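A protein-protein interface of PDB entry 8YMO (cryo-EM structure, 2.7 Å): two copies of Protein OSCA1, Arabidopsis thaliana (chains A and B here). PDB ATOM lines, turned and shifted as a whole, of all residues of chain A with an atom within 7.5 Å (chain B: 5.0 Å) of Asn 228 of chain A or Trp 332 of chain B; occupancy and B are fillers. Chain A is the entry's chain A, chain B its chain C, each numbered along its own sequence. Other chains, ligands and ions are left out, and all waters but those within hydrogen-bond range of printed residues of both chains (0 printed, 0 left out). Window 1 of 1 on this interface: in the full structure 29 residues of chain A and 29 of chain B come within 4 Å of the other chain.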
ATOM      1  N   GLU A 222      28.327 -22.111 -10.117  1.00  0.00           N
ATOM      2  CA  GLU A 222      27.270 -21.947 -11.102  1.00  0.00           C
ATOM      3  C   GLU A 222      26.420 -20.741 -10.775  1.00  0.00           C
ATOM      4  O   GLU A 222      26.249 -19.862 -11.609  1.00  0.00           O
ATOM      5  CB  GLU A 222      26.394 -23.194 -11.162  1.00  0.00           C
ATOM      6  CG  GLU A 222      25.274 -23.123 -12.184  1.00  0.00           C
ATOM      7  CD  GLU A 222      25.446 -24.127 -13.303  1.00  0.00           C
ATOM      8  OE1 GLU A 222      25.996 -25.216 -13.044  1.00  0.00           O
ATOM      9  OE2 GLU A 222      25.033 -23.828 -14.442  1.00  0.00           O
ATOM     10  N   HIS A 223      25.903 -20.680  -9.554  1.00  0.00           N
ATOM     11  CA  HIS A 223      25.023 -19.583  -9.168  1.00  0.00           C
ATOM     12  C   HIS A 223      25.697 -18.223  -9.245  1.00  0.00           C
ATOM     13  O   HIS A 223      25.087 -17.266  -9.694  1.00  0.00           O
ATOM     14  CB  HIS A 223      24.402 -19.846  -7.785  1.00  0.00           C
ATOM     15  CG  HIS A 223      24.699 -18.791  -6.764  1.00  0.00           C
ATOM     16  ND1 HIS A 223      23.973 -17.623  -6.664  1.00  0.00           N
ATOM     17  CD2 HIS A 223      25.634 -18.737  -5.785  1.00  0.00           C
ATOM     18  CE1 HIS A 223      24.457 -16.890  -5.678  1.00  0.00           C
ATOM     19  NE2 HIS A 223      25.465 -17.543  -5.129  1.00  0.00           N
ATOM     20  N   PHE A 224      26.954 -18.135  -8.826  1.00  0.00           N
ATOM     21  CA  PHE A 224      27.672 -16.872  -8.873  1.00  0.00           C
ATOM     22  C   PHE A 224      27.780 -16.377 -10.287  1.00  0.00           C
ATOM     23  O   PHE A 224      27.429 -15.245 -10.577  1.00  0.00           O
ATOM     24  CB  PHE A 224      29.074 -17.031  -8.305  1.00  0.00           C
ATOM     25  CG  PHE A 224      29.819 -15.736  -8.139  1.00  0.00           C
ATOM     26  CD1 PHE A 224      29.707 -15.006  -6.971  1.00  0.00           C
ATOM     27  CD2 PHE A 224      30.643 -15.257  -9.144  1.00  0.00           C
ATOM     28  CE1 PHE A 224      30.392 -13.819  -6.812  1.00  0.00           C
ATOM     29  CE2 PHE A 224      31.328 -14.071  -8.993  1.00  0.00           C
ATOM     30  CZ  PHE A 224      31.202 -13.352  -7.823  1.00  0.00           C
ATOM     31  N   PHE A 225      28.259 -17.220 -11.185  1.00  0.00           N
ATOM     32  CA  PHE A 225      28.481 -16.773 -12.547  1.00  0.00           C
ATOM     33  C   PHE A 225      27.218 -16.755 -13.382  1.00  0.00           C
ATOM     34  O   PHE A 225      27.245 -16.327 -14.521  1.00  0.00           O
ATOM     35  CB  PHE A 225      29.589 -17.596 -13.198  1.00  0.00           C
ATOM     36  CG  PHE A 225      30.935 -17.371 -12.579  1.00  0.00           C
ATOM     37  CD1 PHE A 225      31.756 -16.361 -13.036  1.00  0.00           C
ATOM     38  CD2 PHE A 225      31.369 -18.152 -11.525  1.00  0.00           C
ATOM     39  CE1 PHE A 225      32.989 -16.144 -12.460  1.00  0.00           C
ATOM     40  CE2 PHE A 225      32.599 -17.939 -10.944  1.00  0.00           C
ATOM     41  CZ  PHE A 225      33.413 -16.933 -11.414  1.00  0.00           C
ATOM     42  N   LEU A 226      26.103 -17.198 -12.824  1.00  0.00           N
ATOM     43  CA  LEU A 226      24.843 -17.119 -13.544  1.00  0.00           C
ATOM     44  C   LEU A 226      24.135 -15.837 -13.154  1.00  0.00           C
ATOM     45  O   LEU A 226      23.226 -15.391 -13.847  1.00  0.00           O
ATOM     46  CB  LEU A 226      23.958 -18.323 -13.232  1.00  0.00           C
ATOM     47  CG  LEU A 226      23.153 -18.943 -14.374  1.00  0.00           C
ATOM     48  CD1 LEU A 226      23.571 -18.387 -15.726  1.00  0.00           C
ATOM     49  CD2 LEU A 226      23.281 -20.456 -14.343  1.00  0.00           C
ATOM     50  N   VAL A 227      24.538 -15.242 -12.038  1.00  0.00           N
ATOM     51  CA  VAL A 227      23.947 -13.977 -11.627  1.00  0.00           C
ATOM     52  C   VAL A 227      24.884 -12.799 -11.862  1.00  0.00           C
ATOM     53  O   VAL A 227      24.423 -11.681 -12.060  1.00  0.00           O
ATOM     54  CB  VAL A 227      23.448 -13.997 -10.161  1.00  0.00           C
ATOM     55  CG1 VAL A 227      22.494 -15.156  -9.931  1.00  0.00           C
ATOM     56  CG2 VAL A 227      24.595 -14.024  -9.167  1.00  0.00           C
ATOM     57  N   ASN A 228      26.190 -13.038 -11.861  1.00  0.00           N
ATOM     58  CA  ASN A 228      27.145 -11.947 -12.017  1.00  0.00           C
ATOM     59  C   ASN A 228      27.657 -11.874 -13.433  1.00  0.00           C
ATOM     60  O   ASN A 228      28.086 -10.814 -13.878  1.00  0.00           O
ATOM     61  CB  ASN A 228      28.287 -12.072 -11.016  1.00  0.00           C
ATOM     62  CG  ASN A 228      27.836 -11.826  -9.594  1.00  0.00           C
ATOM     63  OD1 ASN A 228      27.778 -12.744  -8.782  1.00  0.00           O
ATOM     64  ND2 ASN A 228      27.504 -10.581  -9.290  1.00  0.00           N
ATOM     65  N   HIS A 229      27.621 -12.987 -14.152  1.00  0.00           N
ATOM     66  CA  HIS A 229      28.002 -12.982 -15.560  1.00  0.00           C
ATOM     67  C   HIS A 229      26.906 -13.717 -16.287  1.00  0.00           C
ATOM     68  O   HIS A 229      27.165 -14.729 -16.922  1.00  0.00           O
ATOM     69  CB  HIS A 229      29.324 -13.706 -15.762  1.00  0.00           C
ATOM     70  CG  HIS A 229      30.510 -12.954 -15.248  1.00  0.00           C
ATOM     71  ND1 HIS A 229      31.217 -12.063 -16.025  1.00  0.00           N
ATOM     72  CD2 HIS A 229      31.112 -12.959 -14.037  1.00  0.00           C
ATOM     73  CE1 HIS A 229      32.203 -11.549 -15.313  1.00  0.00           C
ATOM     74  NE2 HIS A 229      32.163 -12.078 -14.104  1.00  0.00           N
ATOM     75  N   PRO A 230      25.669 -13.201 -16.230  1.00  0.00           N
ATOM     76  CA  PRO A 230      24.550 -13.953 -16.805  1.00  0.00           C
ATOM     77  C   PRO A 230      24.583 -14.112 -18.305  1.00  0.00           C
ATOM     78  O   PRO A 230      24.402 -15.222 -18.799  1.00  0.00           O
ATOM     79  CB  PRO A 230      23.331 -13.098 -16.432  1.00  0.00           C
ATOM     80  CG  PRO A 230      23.831 -11.980 -15.576  1.00  0.00           C
ATOM     81  CD  PRO A 230      25.274 -11.820 -15.915  1.00  0.00           C
ATOM     82  N   ASP A 231      24.804 -13.027 -19.026  1.00  0.00           N
ATOM     83  CA  ASP A 231      24.760 -13.068 -20.478  1.00  0.00           C
ATOM     84  C   ASP A 231      25.601 -14.143 -21.131  1.00  0.00           C
ATOM     85  O   ASP A 231      25.140 -14.807 -22.055  1.00  0.00           O
ATOM     86  CB  ASP A 231      25.152 -11.699 -21.035  1.00  0.00           C
ATOM     87  CG  ASP A 231      25.985 -10.891 -20.056  1.00  0.00           C
ATOM     88  OD1 ASP A 231      27.131 -11.296 -19.763  1.00  0.00           O
ATOM     89  OD2 ASP A 231      25.493  -9.847 -19.577  1.00  0.00           O
ATOM     90  N   ASN A 232      26.832 -14.331 -20.671  1.00  0.00           N
ATOM     91  CA  ASN A 232      27.705 -15.270 -21.358  1.00  0.00           C
ATOM     92  C   ASN A 232      28.354 -16.358 -20.528  1.00  0.00           C
ATOM     93  O   ASN A 232      29.460 -16.755 -20.832  1.00  0.00           O
ATOM     94  CB  ASN A 232      28.791 -14.505 -22.108  1.00  0.00           C
ATOM     95  CG  ASN A 232      28.248 -13.712 -23.275  1.00  0.00           C
ATOM     96  OD1 ASN A 232      27.732 -14.276 -24.239  1.00  0.00           O
ATOM     97  ND2 ASN A 232      28.365 -12.392 -23.196  1.00  0.00           N
ATOM     98  N   TYR A 233      27.684 -16.864 -19.505  1.00  0.00           N
ATOM     99  CA  TYR A 233      28.238 -17.984 -18.756  1.00  0.00           C
ATOM    100  C   TYR A 233      27.784 -19.272 -19.411  1.00  0.00           C
ATOM    101  O   TYR A 233      26.595 -19.461 -19.646  1.00  0.00           O
ATOM    102  CB  TYR A 233      27.788 -17.946 -17.300  1.00  0.00           C
ATOM    103  CG  TYR A 233      27.924 -19.254 -16.558  1.00  0.00           C
ATOM    104  CD1 TYR A 233      29.170 -19.759 -16.224  1.00  0.00           C
ATOM    105  CD2 TYR A 233      26.806 -19.982 -16.184  1.00  0.00           C
ATOM    106  CE1 TYR A 233      29.295 -20.953 -15.545  1.00  0.00           C
ATOM    107  CE2 TYR A 233      26.924 -21.176 -15.507  1.00  0.00           C
ATOM    108  CZ  TYR A 233      28.172 -21.656 -15.190  1.00  0.00           C
ATOM    109  OH  TYR A 233      28.295 -22.845 -14.517  1.00  0.00           O
ATOM    110  N   PHE A 328      33.053 -19.665 -20.625  1.00  0.00           N
ATOM    111  CA  PHE A 328      32.097 -18.674 -21.067  1.00  0.00           C
ATOM    112  C   PHE A 328      31.767 -18.883 -22.529  1.00  0.00           C
ATOM    113  O   PHE A 328      32.517 -19.530 -23.247  1.00  0.00           O
ATOM    114  CB  PHE A 328      32.659 -17.276 -20.838  1.00  0.00           C
ATOM    115  CG  PHE A 328      32.782 -16.903 -19.390  1.00  0.00           C
ATOM    116  CD1 PHE A 328      31.716 -16.344 -18.714  1.00  0.00           C
ATOM    117  CD2 PHE A 328      33.963 -17.114 -18.705  1.00  0.00           C
ATOM    118  CE1 PHE A 328      31.820 -16.003 -17.385  1.00  0.00           C
ATOM    119  CE2 PHE A 328      34.076 -16.775 -17.376  1.00  0.00           C
ATOM    120  CZ  PHE A 328      33.001 -16.220 -16.714  1.00  0.00           C
ATOM    121  N   TRP A 332      35.264 -12.813 -25.104  1.00  0.00           N
ATOM    122  CA  TRP A 332      35.094 -11.479 -24.561  1.00  0.00           C
ATOM    123  C   TRP A 332      34.632 -11.585 -23.125  1.00  0.00           C
ATOM    124  O   TRP A 332      35.084 -10.832 -22.273  1.00  0.00           O
ATOM    125  CB  TRP A 332      34.063 -10.735 -25.410  1.00  0.00           C
ATOM    126  CG  TRP A 332      33.809  -9.314 -25.045  1.00  0.00           C
ATOM    127  CD1 TRP A 332      34.416  -8.216 -25.570  1.00  0.00           C
ATOM    128  CD2 TRP A 332      32.847  -8.829 -24.103  1.00  0.00           C
ATOM    129  NE1 TRP A 332      33.905  -7.076 -25.003  1.00  0.00           N
ATOM    130  CE2 TRP A 332      32.941  -7.426 -24.096  1.00  0.00           C
ATOM    131  CE3 TRP A 332      31.920  -9.447 -23.258  1.00  0.00           C
ATOM    132  CZ2 TRP A 332      32.147  -6.631 -23.277  1.00  0.00           C
ATOM    133  CZ3 TRP A 332      31.138  -8.658 -22.445  1.00  0.00           C
ATOM    134  CH2 TRP A 332      31.253  -7.265 -22.460  1.00  0.00           C
ATOM    135  N   ALA A 333      33.740 -12.525 -22.846  1.00  0.00           N
ATOM    136  CA  ALA A 333      33.234 -12.706 -21.496  1.00  0.00           C
ATOM    137  C   ALA A 333      34.298 -13.231 -20.571  1.00  0.00           C
ATOM    138  O   ALA A 333      34.358 -12.847 -19.410  1.00  0.00           O
ATOM    139  CB  ALA A 333      32.064 -13.652 -21.512  1.00  0.00           C
ATOM    140  N   VAL A 336      36.558 -10.334 -19.824  1.00  0.00           N
ATOM    141  CA  VAL A 336      35.921  -9.528 -18.798  1.00  0.00           C
ATOM    142  C   VAL A 336      36.130 -10.162 -17.436  1.00  0.00           C
ATOM    143  O   VAL A 336      36.671  -9.531 -16.543  1.00  0.00           O
ATOM    144  CB  VAL A 336      34.423  -9.334 -19.085  1.00  0.00           C
ATOM    145  CG1 VAL A 336      33.687  -8.854 -17.844  1.00  0.00           C
ATOM    146  CG2 VAL A 336      34.238  -8.341 -20.217  1.00  0.00           C
ATOM    147  N   CYS A 337      35.747 -11.422 -17.280  1.00  0.00           N
ATOM    148  CA  CYS A 337      35.883 -12.089 -15.997  1.00  0.00           C
ATOM    149  C   CYS A 337      37.312 -12.088 -15.476  1.00  0.00           C
ATOM    150  O   CYS A 337      37.548 -11.774 -14.317  1.00  0.00           O
ATOM    151  CB  CYS A 337      35.355 -13.510 -16.086  1.00  0.00           C
ATOM    152  SG  CYS A 337      35.031 -14.271 -14.490  1.00  0.00           S
ATOM    153  N   THR A 340      38.493  -8.481 -14.263  1.00  0.00           N
ATOM    154  CA  THR A 340      37.556  -7.717 -13.454  1.00  0.00           C
ATOM    155  C   THR A 340      37.474  -8.287 -12.044  1.00  0.00           C
ATOM    156  O   THR A 340      37.723  -9.474 -11.837  1.00  0.00           O
ATOM    157  CB  THR A 340      36.167  -7.619 -14.135  1.00  0.00           C
ATOM    158  OG1 THR A 340      35.668  -6.281 -14.026  1.00  0.00           O
ATOM    159  CG2 THR A 340      35.161  -8.583 -13.531  1.00  0.00           C
ATOM    160  N   THR A 341      37.175  -7.440 -11.064  1.00  0.00           N
ATOM    161  CA  THR A 341      37.020  -7.913  -9.694  1.00  0.00           C
ATOM    162  C   THR A 341      35.594  -8.373  -9.520  1.00  0.00           C
ATOM    163  O   THR A 341      34.669  -7.719  -9.987  1.00  0.00           O
ATOM    164  CB  THR A 341      37.392  -6.838  -8.656  1.00  0.00           C
ATOM    165  OG1 THR A 341      36.743  -7.125  -7.411  1.00  0.00           O
ATOM    166  CG2 THR A 341      36.982  -5.458  -9.136  1.00  0.00           C
ATOM    167  N   GLN A 342      35.401  -9.501  -8.854  1.00  0.00           N
ATOM    168  CA  GLN A 342      34.065 -10.063  -8.746  1.00  0.00           C
ATOM    169  C   GLN A 342      33.340  -9.747  -7.463  1.00  0.00           C
ATOM    170  O   GLN A 342      32.144  -9.481  -7.480  1.00  0.00           O
ATOM    171  CB  GLN A 342      34.148 -11.577  -8.914  1.00  0.00           C
ATOM    172  CG  GLN A 342      35.119 -12.031  -9.983  1.00  0.00           C
ATOM    173  CD  GLN A 342      34.524 -11.936 -11.367  1.00  0.00           C
ATOM    174  OE1 GLN A 342      33.317 -12.075 -11.544  1.00  0.00           O
ATOM    175  NE2 GLN A 342      35.367 -11.694 -12.355  1.00  0.00           N
ATOM    176  N   THR A 343      34.044  -9.783  -6.345  1.00  0.00           N
ATOM    177  CA  THR A 343      33.393  -9.578  -5.065  1.00  0.00           C
ATOM    178  C   THR A 343      34.144  -8.559  -4.224  1.00  0.00           C
ATOM    179  O   THR A 343      35.260  -8.178  -4.567  1.00  0.00           O
ATOM    180  CB  THR A 343      33.257 -10.921  -4.318  1.00  0.00           C
ATOM    181  OG1 THR A 343      32.765 -10.703  -2.991  1.00  0.00           O
ATOM    182  CG2 THR A 343      34.589 -11.621  -4.246  1.00  0.00           C
ATOM    183  N   TRP A 349      36.867 -15.491  -4.842  1.00  0.00           N
ATOM    184  CA  TRP A 349      36.449 -15.509  -6.239  1.00  0.00           C
ATOM    185  C   TRP A 349      37.524 -14.889  -7.109  1.00  0.00           C
ATOM    186  O   TRP A 349      37.239 -14.008  -7.913  1.00  0.00           O
ATOM    187  CB  TRP A 349      35.118 -14.786  -6.442  1.00  0.00           C
ATOM    188  CG  TRP A 349      33.951 -15.405  -5.744  1.00  0.00           C
ATOM    189  CD1 TRP A 349      33.357 -14.962  -4.602  1.00  0.00           C
ATOM    190  CD2 TRP A 349      33.218 -16.567  -6.150  1.00  0.00           C
ATOM    191  NE1 TRP A 349      32.303 -15.773  -4.270  1.00  0.00           N
ATOM    192  CE2 TRP A 349      32.200 -16.770  -5.203  1.00  0.00           C
ATOM    193  CE3 TRP A 349      33.324 -17.453  -7.223  1.00  0.00           C
ATOM    194  CZ2 TRP A 349      31.299 -17.825  -5.292  1.00  0.00           C
ATOM    195  CZ3 TRP A 349      32.431 -18.497  -7.308  1.00  0.00           C
ATOM    196  CH2 TRP A 349      31.432 -18.676  -6.350  1.00  0.00           C
ATOM    197  N   ASN B 232      25.386  -3.756 -23.339  1.00  0.00           N
ATOM    198  CA  ASN B 232      24.958  -2.701 -22.434  1.00  0.00           C
ATOM    199  C   ASN B 232      25.490  -1.305 -22.685  1.00  0.00           C
ATOM    200  O   ASN B 232      25.688  -0.568 -21.741  1.00  0.00           O
ATOM    201  CB  ASN B 232      25.273  -3.101 -20.996  1.00  0.00           C
ATOM    202  CG  ASN B 232      24.427  -4.256 -20.511  1.00  0.00           C
ATOM    203  OD1 ASN B 232      23.207  -4.144 -20.399  1.00  0.00           O
ATOM    204  ND2 ASN B 232      25.074  -5.377 -20.215  1.00  0.00           N
ATOM    205  N   THR B 330      23.915  -0.514 -17.507  1.00  0.00           N
ATOM    206  CA  THR B 330      24.063  -1.061 -16.171  1.00  0.00           C
ATOM    207  C   THR B 330      25.343  -0.572 -15.524  1.00  0.00           C
ATOM    208  O   THR B 330      26.241  -0.094 -16.207  1.00  0.00           O
ATOM    209  CB  THR B 330      24.073  -2.598 -16.205  1.00  0.00           C
ATOM    210  OG1 THR B 330      24.868  -3.050 -17.305  1.00  0.00           O
ATOM    211  CG2 THR B 330      22.665  -3.146 -16.351  1.00  0.00           C
ATOM    212  N   ARG B 331      25.433  -0.682 -14.205  1.00  0.00           N
ATOM    213  CA  ARG B 331      26.647  -0.299 -13.505  1.00  0.00           C
ATOM    214  C   ARG B 331      27.629  -1.425 -13.671  1.00  0.00           C
ATOM    215  O   ARG B 331      28.831  -1.217 -13.573  1.00  0.00           O
ATOM    216  CB  ARG B 331      26.364  -0.103 -12.022  1.00  0.00           C
ATOM    217  CG  ARG B 331      25.412   1.028 -11.710  1.00  0.00           C
ATOM    218  CD  ARG B 331      25.052   1.035 -10.240  1.00  0.00           C
ATOM    219  NE  ARG B 331      23.654   0.690 -10.033  1.00  0.00           N
ATOM    220  CZ  ARG B 331      22.707   1.571  -9.736  1.00  0.00           C
ATOM    221  NH1 ARG B 331      23.006   2.853  -9.607  1.00  0.00           N
ATOM    222  NH2 ARG B 331      21.463   1.169  -9.559  1.00  0.00           N
ATOM    223  N   TRP B 332      27.119  -2.624 -13.918  1.00  0.00           N
ATOM    224  CA  TRP B 332      27.968  -3.782 -14.128  1.00  0.00           C
ATOM    225  C   TRP B 332      28.759  -3.591 -15.402  1.00  0.00           C
ATOM    226  O   TRP B 332      29.936  -3.918 -15.455  1.00  0.00           O
ATOM    227  CB  TRP B 332      27.083  -5.025 -14.219  1.00  0.00           C
ATOM    228  CG  TRP B 332      27.788  -6.329 -14.363  1.00  0.00           C
ATOM    229  CD1 TRP B 332      28.153  -7.174 -13.360  1.00  0.00           C
ATOM    230  CD2 TRP B 332      28.180  -6.962 -15.584  1.00  0.00           C
ATOM    231  NE1 TRP B 332      28.762  -8.288 -13.880  1.00  0.00           N
ATOM    232  CE2 TRP B 332      28.794  -8.180 -15.244  1.00  0.00           C
ATOM    233  CE3 TRP B 332      28.079  -6.612 -16.934  1.00  0.00           C
ATOM    234  CZ2 TRP B 332      29.305  -9.049 -16.202  1.00  0.00           C
ATOM    235  CZ3 TRP B 332      28.589  -7.472 -17.880  1.00  0.00           C
ATOM    236  CH2 TRP B 332      29.193  -8.678 -17.512  1.00  0.00           C
ATOM    237  N   ALA B 333      28.123  -3.049 -16.432  1.00  0.00           N
ATOM    238  CA  ALA B 333      28.795  -2.824 -17.699  1.00  0.00           C
ATOM    239  C   ALA B 333      29.842  -1.749 -17.588  1.00  0.00           C
ATOM    240  O   ALA B 333      30.898  -1.842 -18.202  1.00  0.00           O
ATOM    241  CB  ALA B 333      27.790  -2.445 -18.751  1.00  0.00           C
ATOM    242  N   ALA B 334      29.552  -0.717 -16.813  1.00  0.00           N
ATOM    243  CA  ALA B 334      30.507   0.352 -16.624  1.00  0.00           C
ATOM    244  C   ALA B 334      31.675  -0.152 -15.818  1.00  0.00           C
ATOM    245  O   ALA B 334      32.804   0.246 -16.054  1.00  0.00           O
ATOM    246  CB  ALA B 334      29.850   1.518 -15.934  1.00  0.00           C
ATOM    247  N   ALA B 335      31.411  -1.035 -14.864  1.00  0.00           N
ATOM    248  CA  ALA B 335      32.481  -1.622 -14.083  1.00  0.00           C
ATOM    249  C   ALA B 335      33.353  -2.421 -15.009  1.00  0.00           C
ATOM    250  O   ALA B 335      34.555  -2.231 -15.030  1.00  0.00           O
ATOM    251  CB  ALA B 335      31.917  -2.501 -12.989  1.00  0.00           C
ATOM    252  N   VAL B 336      32.750  -3.299 -15.799  1.00  0.00           N
ATOM    253  CA  VAL B 336      33.503  -4.075 -16.768  1.00  0.00           C
ATOM    254  C   VAL B 336      34.383  -3.157 -17.596  1.00  0.00           C
ATOM    255  O   VAL B 336      35.590  -3.332 -17.632  1.00  0.00           O
ATOM    256  CB  VAL B 336      32.575  -4.902 -17.673  1.00  0.00           C
ATOM    257  CG1 VAL B 336      33.307  -5.382 -18.915  1.00  0.00           C
ATOM    258  CG2 VAL B 336      32.023  -6.086 -16.901  1.00  0.00           C
ATOM    259  N   LEU B 686      32.105  -6.522  -9.326  1.00  0.00           N
ATOM    260  CA  LEU B 686      31.023  -6.796 -10.267  1.00  0.00           C
ATOM    261  C   LEU B 686      29.784  -7.354  -9.590  1.00  0.00           C
ATOM    262  O   LEU B 686      28.676  -7.144 -10.065  1.00  0.00           O
ATOM    263  CB  LEU B 686      31.508  -7.749 -11.362  1.00  0.00           C
ATOM    264  CG  LEU B 686      31.874  -7.171 -12.730  1.00  0.00           C
ATOM    265  CD1 LEU B 686      32.900  -6.059 -12.616  1.00  0.00           C
ATOM    266  CD2 LEU B 686      32.387  -8.277 -13.636  1.00  0.00           C
ATOM    267  N   GLN B 687      29.961  -8.059  -8.481  1.00  0.00           N
ATOM    268  CA  GLN B 687      28.822  -8.575  -7.740  1.00  0.00           C
ATOM    269  C   GLN B 687      28.063  -7.426  -7.124  1.00  0.00           C
ATOM    270  O   GLN B 687      26.840  -7.396  -7.157  1.00  0.00           O
ATOM    271  CB  GLN B 687      29.284  -9.530  -6.649  1.00  0.00           C
ATOM    272  CG  GLN B 687      28.172 -10.374  -6.056  1.00  0.00           C
ATOM    273  CD  GLN B 687      28.535 -10.932  -4.697  1.00  0.00           C
ATOM    274  OE1 GLN B 687      28.107 -12.023  -4.329  1.00  0.00           O
ATOM    275  NE2 GLN B 687      29.331 -10.183  -3.944  1.00  0.00           N
ATOM    276  N   ALA B 689      28.013  -4.348  -8.190  1.00  0.00           N
ATOM    277  CA  ALA B 689      27.370  -3.632  -9.277  1.00  0.00           C
ATOM    278  C   ALA B 689      26.092  -4.320  -9.697  1.00  0.00           C
ATOM    279  O   ALA B 689      25.067  -3.672  -9.858  1.00  0.00           O
ATOM    280  CB  ALA B 689      28.318  -3.527 -10.448  1.00  0.00           C
ATOM    281  N   MET B 690      26.142  -5.635  -9.862  1.00  0.00           N
ATOM    282  CA  MET B 690      24.967  -6.387 -10.271  1.00  0.00           C
ATOM    283  C   MET B 690      23.866  -6.354  -9.224  1.00  0.00           C
ATOM    284  O   MET B 690      22.694  -6.263  -9.564  1.00  0.00           O
ATOM    285  CB  MET B 690      25.342  -7.830 -10.606  1.00  0.00           C
ATOM    286  CG  MET B 690      24.263  -8.601 -11.346  1.00  0.00           C
ATOM    287  SD  MET B 690      24.442  -8.508 -13.135  1.00  0.00           S
ATOM    288  CE  MET B 690      23.218  -7.266 -13.542  1.00  0.00           C
ATOM    289  N   ASP B 693      22.202  -3.026  -9.474  1.00  0.00           N
ATOM    290  CA  ASP B 693      21.427  -2.979 -10.704  1.00  0.00           C
ATOM    291  C   ASP B 693      20.117  -3.717 -10.568  1.00  0.00           C
ATOM    292  O   ASP B 693      19.071  -3.189 -10.923  1.00  0.00           O
ATOM    293  CB  ASP B 693      22.226  -3.576 -11.857  1.00  0.00           C
ATOM    294  CG  ASP B 693      23.251  -2.622 -12.404  1.00  0.00           C
ATOM    295  OD1 ASP B 693      22.953  -1.414 -12.491  1.00  0.00           O
ATOM    296  OD2 ASP B 693      24.357  -3.081 -12.750  1.00  0.00           O
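The indole nitrogen (NE1) of Trp 332 of chain B lies within hydrogen-bond range of the backbone carbonyl oxygen (O) of Asn 228 of chain A. The backbone carbonyl oxygen (O) of Thr 341 of chain A lies within hydrogen-bond range of the backbone NH (N) of Leu 686 of chain B, 2.9 Å away. O of Gln 342 of chain A sits at hydrogen-bond distance from N of Leu 686 of chain B. The backbone carbonyl oxygen (O) of Gln 342 of chain A sits at hydrogen-bond distance from the backbone NH (N) of Gln 687 of chain B (2.8 Å). The backbone carbonyl oxygen of Val 227 of chain A sits close to the side-chain sulfur of Met 690 of chain B.
The backbone carbonyl oxygen of Phe 224 of chain A lies close to the side-chain amide oxygen of Asn 228 of chain A. A ring nitrogen (NE2) of His 229 of chain A is in hydrogen-bond range of the side-chain amide oxygen (OE1) of Gln 342 of chain A, 2.8 Å away. The side-chain amide nitrogen of Gln 342 of chain A is in hydrogen-bond range of the backbone carbonyl oxygen of Cys 337 of chain A, 2.9 Å away. The backbone carbonyl oxygen of Thr 340 of chain A is in hydrogen-bond range of the side-chain amide nitrogen of Gln 342 of chain A, at 3.3 Å. OG1 of Thr 341 of chain A is in hydrogen-bond range of O of Thr 343 of chain A (3.4 Å). The backbone NH (N) of Trp 332 of chain B sits at hydrogen-bond distance from the side-chain carboxylate (OD2) of Asp 693 of chain B, 3.0 Å away.
Among the printed residues, pairs that only touch across the chains: Thr 340 of chain A with Leu 686 of chain B (2.8 Å), Asn 228 of chain A with Gln 687 of chain B (2.9 Å), Val 336 of chain A with Val 336 of chain B (3.4 Å), His 229 of chain A with Trp 332 of chain B (3.6 Å), Thr 343 of chain A with Gln 687 of chain B (3.6 Å), His 229 of chain A with Leu 686 of chain B (3.7 Å), Asn 228 of chain A with Leu 686 of chain B (3.7 Å), Asn 228 of chain A with Met 690 of chain B (3.7 Å) and Phe 224 of chain A with Gln 687 of chain B (3.8 Å).
Printed residues of chain B within 4 Å of Phe 224 of chain A: Gln 687 (3.8 Å). Of chain B, only Trp 332 (2.6 Å), Leu 686 (3.7 Å), Gln 687 (2.9 Å) and Met 690 (3.7 Å) come within 4 Å of Asn 228 of chain A. Trp 332 of chain B touches just these residues of chain A: Asn 228 (2.6 Å) and His 229 (3.6 Å). Ala 333 of chain B touches none of the printed residues of chain A. Printed residues of chain A within 4 Å of Val 336 of chain B: Val 336 (3.4 Å). Printed residues of chain A within 4 Å of Leu 686 of chain B: Asn 228 (3.7 Å), His 229 (3.7 Å), Thr 340 (2.8 Å), Thr 341 (2.9 Å) and Gln 342 (3.5 Å). The nearest printed residue of chain B that does not touch Asn 228 of chain A is Ala 689 of chain B (6.3 Å). The nearest printed residue of chain B that does not touch His 229 of chain A is Met 690 of chain B (5.6 Å).
Of the 13 printed residues of chain B, 5 touch a printed residue of chain A. Of the 22 printed residues of chain A, 9 touch a printed residue of chain B. Printed residues of chain A that touch a printed residue of chain B: Phe 224, Val 227, Asn 228, His 229, Val 336, Thr 340, Thr 341, Gln 342 and Thr 343.
Val 336 of chain B touches its own counterpart, Val 336 of chain A.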
